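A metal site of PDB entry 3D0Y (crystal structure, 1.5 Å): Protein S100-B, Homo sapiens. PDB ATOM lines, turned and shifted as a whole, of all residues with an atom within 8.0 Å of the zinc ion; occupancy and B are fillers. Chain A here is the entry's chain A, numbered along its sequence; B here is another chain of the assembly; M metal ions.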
ATOM      1  N   HIS A  86     -24.935  -3.827  22.007  1.00  0.00           N
ATOM      2  CA  HIS A  86     -24.581  -4.429  20.743  1.00  0.00           C
ATOM      3  C   HIS A  86     -25.338  -3.777  19.594  1.00  0.00           C
ATOM      4  O   HIS A  86     -24.709  -3.231  18.680  1.00  0.00           O
ATOM      5  CB  HIS A  86     -24.845  -5.948  20.777  1.00  0.00           C
ATOM      6  CG  HIS A  86     -24.467  -6.625  19.507  1.00  0.00           C
ATOM      7  ND1 HIS A  86     -25.329  -7.433  18.799  1.00  0.00           N
ATOM      8  CD2 HIS A  86     -23.315  -6.603  18.796  1.00  0.00           C
ATOM      9  CE1 HIS A  86     -24.726  -7.876  17.709  1.00  0.00           C
ATOM     10  NE2 HIS A  86     -23.498  -7.398  17.690  1.00  0.00           N
ATOM     11  N   GLU A  87     -26.657  -3.782  19.656  1.00  0.00           N
ATOM     12  CA  GLU A  87     -27.504  -3.267  18.593  1.00  0.00           C
ATOM     13  C   GLU A  87     -27.369  -1.773  18.425  1.00  0.00           C
ATOM     14  O   GLU A  87     -27.311  -1.282  17.309  1.00  0.00           O
ATOM     15  CB  GLU A  87     -29.026  -3.564  18.830  1.00  0.00           C
ATOM     16  CG  GLU A  87     -29.424  -4.928  19.449  1.00  0.00           C
ATOM     17  CD  GLU A  87     -29.354  -6.099  18.493  1.00  0.00           C
ATOM     18  OE1 GLU A  87     -28.601  -6.013  17.514  1.00  0.00           O
ATOM     19  OE2 GLU A  87     -30.055  -7.128  18.758  1.00  0.00           O
ATOM     20  N   PHE A  89     -25.049   0.390  19.087  1.00  0.00           N
ATOM     21  CA  PHE A  89     -23.786   0.972  18.660  1.00  0.00           C
ATOM     22  C   PHE A  89     -23.326   0.512  17.269  1.00  0.00           C
ATOM     23  O   PHE A  89     -22.277   0.910  16.775  1.00  0.00           O
ATOM     24  CB  PHE A  89     -22.738   0.788  19.751  1.00  0.00           C
ATOM     25  CG  PHE A  89     -22.924   1.710  20.957  1.00  0.00           C
ATOM     26  CD1 PHE A  89     -23.217   1.207  22.209  1.00  0.00           C
ATOM     27  CD2 PHE A  89     -22.799   3.100  20.791  1.00  0.00           C
ATOM     28  CE1 PHE A  89     -23.389   2.068  23.315  1.00  0.00           C
ATOM     29  CE2 PHE A  89     -22.969   3.968  21.876  1.00  0.00           C
ATOM     30  CZ  PHE A  89     -23.262   3.435  23.142  1.00  0.00           C
ATOM     31  N   GLU A  90     -24.148  -0.276  16.598  1.00  0.00           N
ATOM     32  CA  GLU A  90     -23.827  -0.695  15.247  1.00  0.00           C
ATOM     33  C   GLU A  90     -24.715   0.072  14.316  1.00  0.00           C
ATOM     34  O   GLU A  90     -25.852   0.358  14.702  1.00  0.00           O
ATOM     35  CB  GLU A  90     -24.034  -2.206  15.099  1.00  0.00           C
ATOM     36  CG  GLU A  90     -23.043  -2.972  15.899  1.00  0.00           C
ATOM     37  CD  GLU A  90     -22.992  -4.466  15.655  1.00  0.00           C
ATOM     38  OE1 GLU A  90     -21.997  -5.053  16.095  1.00  0.00           O
ATOM     39  OE2 GLU A  90     -23.915  -5.084  15.093  1.00  0.00           O
ATOM     40  N   ILE B  12     -19.074  -8.500  23.809  1.00  0.00           N
ATOM     41  CA  ILE B  12     -19.362  -8.115  22.437  1.00  0.00           C
ATOM     42  C   ILE B  12     -18.052  -8.214  21.607  1.00  0.00           C
ATOM     43  O   ILE B  12     -18.054  -8.765  20.493  1.00  0.00           O
ATOM     44  CB  ILE B  12     -19.907  -6.716  22.412  1.00  0.00           C
ATOM     45  CG1 ILE B  12     -21.264  -6.603  23.169  1.00  0.00           C
ATOM     46  CG2 ILE B  12     -19.951  -6.215  21.010  1.00  0.00           C
ATOM     47  CD1 ILE B  12     -21.580  -5.175  23.548  1.00  0.00           C
ATOM     48  N   PHE B  15     -17.013 -11.969  20.923  1.00  0.00           N
ATOM     49  CA  PHE B  15     -17.969 -12.469  19.927  1.00  0.00           C
ATOM     50  C   PHE B  15     -17.627 -11.998  18.510  1.00  0.00           C
ATOM     51  O   PHE B  15     -17.524 -12.819  17.594  1.00  0.00           O
ATOM     52  CB  PHE B  15     -19.438 -12.124  20.275  1.00  0.00           C
ATOM     53  CG  PHE B  15     -20.432 -12.589  19.223  1.00  0.00           C
ATOM     54  CD1 PHE B  15     -20.894 -13.890  19.199  1.00  0.00           C
ATOM     55  CD2 PHE B  15     -20.847 -11.716  18.204  1.00  0.00           C
ATOM     56  CE1 PHE B  15     -21.804 -14.301  18.165  1.00  0.00           C
ATOM     57  CE2 PHE B  15     -21.744 -12.106  17.172  1.00  0.00           C
ATOM     58  CZ  PHE B  15     -22.236 -13.403  17.172  1.00  0.00           C
ATOM     59  N   HIS B  16     -17.438 -10.681  18.361  1.00  0.00           N
ATOM     60  CA  HIS B  16     -17.033 -10.113  17.074  1.00  0.00           C
ATOM     61  C   HIS B  16     -15.692 -10.685  16.601  1.00  0.00           C
ATOM     62  O   HIS B  16     -15.552 -11.012  15.442  1.00  0.00           O
ATOM     63  CB  HIS B  16     -16.971  -8.591  17.197  1.00  0.00           C
ATOM     64  CG  HIS B  16     -18.293  -7.909  17.051  1.00  0.00           C
ATOM     65  ND1 HIS B  16     -18.651  -6.800  17.807  1.00  0.00           N
ATOM     66  CD2 HIS B  16     -19.321  -8.110  16.182  1.00  0.00           C
ATOM     67  CE1 HIS B  16     -19.859  -6.396  17.450  1.00  0.00           C
ATOM     68  NE2 HIS B  16     -20.272  -7.149  16.447  1.00  0.00           N
ATOM     69  N   SER B  19     -16.669 -14.276  15.350  1.00  0.00           N
ATOM     70  CA  SER B  19     -17.787 -14.335  14.382  1.00  0.00           C
ATOM     71  C   SER B  19     -17.364 -13.739  13.050  1.00  0.00           C
ATOM     72  O   SER B  19     -17.914 -14.068  11.985  1.00  0.00           O
ATOM     73  CB  SER B  19     -19.035 -13.678  14.970  1.00  0.00           C
ATOM     74  OG  SER B  19     -18.953 -12.250  14.876  1.00  0.00           O
ATOM     75  N   LYS B  25     -20.334 -12.634   9.068  1.00  0.00           N
ATOM     76  CA  LYS B  25     -19.386 -11.868   9.884  1.00  0.00           C
ATOM     77  C   LYS B  25     -19.921 -11.565  11.285  1.00  0.00           C
ATOM     78  O   LYS B  25     -19.198 -11.076  12.128  1.00  0.00           O
ATOM     79  CB  LYS B  25     -18.982 -10.561   9.142  1.00  0.00           C
ATOM     80  N   HIS B  26     -21.193 -11.944  11.515  1.00  0.00           N
ATOM     81  CA  HIS B  26     -21.968 -11.567  12.664  1.00  0.00           C
ATOM     82  C   HIS B  26     -22.555 -12.788  13.347  1.00  0.00           C
ATOM     83  O   HIS B  26     -23.391 -12.676  14.237  1.00  0.00           O
ATOM     84  CB  HIS B  26     -23.108 -10.673  12.193  1.00  0.00           C
ATOM     85  CG  HIS B  26     -23.329  -9.473  13.057  1.00  0.00           C
ATOM     86  ND1 HIS B  26     -24.549  -8.821  13.139  1.00  0.00           N
ATOM     87  CD2 HIS B  26     -22.466  -8.770  13.834  1.00  0.00           C
ATOM     88  CE1 HIS B  26     -24.428  -7.781  13.946  1.00  0.00           C
ATOM     89  NE2 HIS B  26     -23.176  -7.734  14.391  1.00  0.00           N
ATOM     90  N   LYS B  27     -22.122 -13.950  12.898  1.00  0.00           N
ATOM     91  CA  LYS B  27     -22.496 -15.193  13.569  1.00  0.00           C
ATOM     92  C   LYS B  27     -21.305 -16.115  13.631  1.00  0.00           C
ATOM     93  O   LYS B  27     -20.396 -15.974  12.806  1.00  0.00           O
ATOM     94  CB  LYS B  27     -23.638 -15.880  12.813  1.00  0.00           C
ATOM     95  CG  LYS B  27     -24.860 -15.039  12.641  1.00  0.00           C
ATOM     96  CD  LYS B  27     -25.965 -15.947  12.252  1.00  0.00           C
ATOM     97  CE  LYS B  27     -27.188 -15.125  12.022  1.00  0.00           C
ATOM     98  NZ  LYS B  27     -27.030 -14.152  10.818  1.00  0.00           N
ATOM     99  N   PHE B  71     -25.537 -13.536  18.138  1.00  0.00           N
ATOM    100  CA  PHE B  71     -25.175 -12.892  19.424  1.00  0.00           C
ATOM    101  C   PHE B  71     -26.065 -13.279  20.597  1.00  0.00           C
ATOM    102  O   PHE B  71     -25.550 -13.576  21.698  1.00  0.00           O
ATOM    103  CB  PHE B  71     -25.134 -11.351  19.333  1.00  0.00           C
ATOM    104  CG  PHE B  71     -24.475 -10.734  20.530  1.00  0.00           C
ATOM    105  CD1 PHE B  71     -23.105 -10.931  20.780  1.00  0.00           C
ATOM    106  CD2 PHE B  71     -25.219  -9.968  21.424  1.00  0.00           C
ATOM    107  CE1 PHE B  71     -22.482 -10.389  21.887  1.00  0.00           C
ATOM    108  CE2 PHE B  71     -24.606  -9.407  22.538  1.00  0.00           C
ATOM    109  CZ  PHE B  71     -23.232  -9.610  22.781  1.00  0.00           C
HETATM  110 ZN    ZN M   1     -22.234  -7.059  15.938  1.00  0.00          ZN
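A ring nitrogen (ND1) of His 16 of chain B is in hydrogen-bond range of the backbone carbonyl oxygen of Ile 12 of chain B, at 3.4 Å.
Of the 12 residues printed, 4 come within 4 Å of the zinc ion.
The nearest printed residue that does not touch the zinc ion is Phe 15 of chain B (5.2 Å).
A ring nitrogen (NE2) of His 26 of chain B binds the zinc ion (1.9 Å).
OE1 of Glu 90 is bound to the zinc ion, at 2.0 Å.
NE2 of His 16 of chain B is bound to the zinc ion, 2.0 Å away.
NE2 of His 86 is bound to the zinc ion (2.2 Å).
The zinc ion has four donor atoms within binding distance.
Slightly farther from the zinc ion lies the side-chain carboxylate (OE2) of Glu 90 (2.7 Å).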
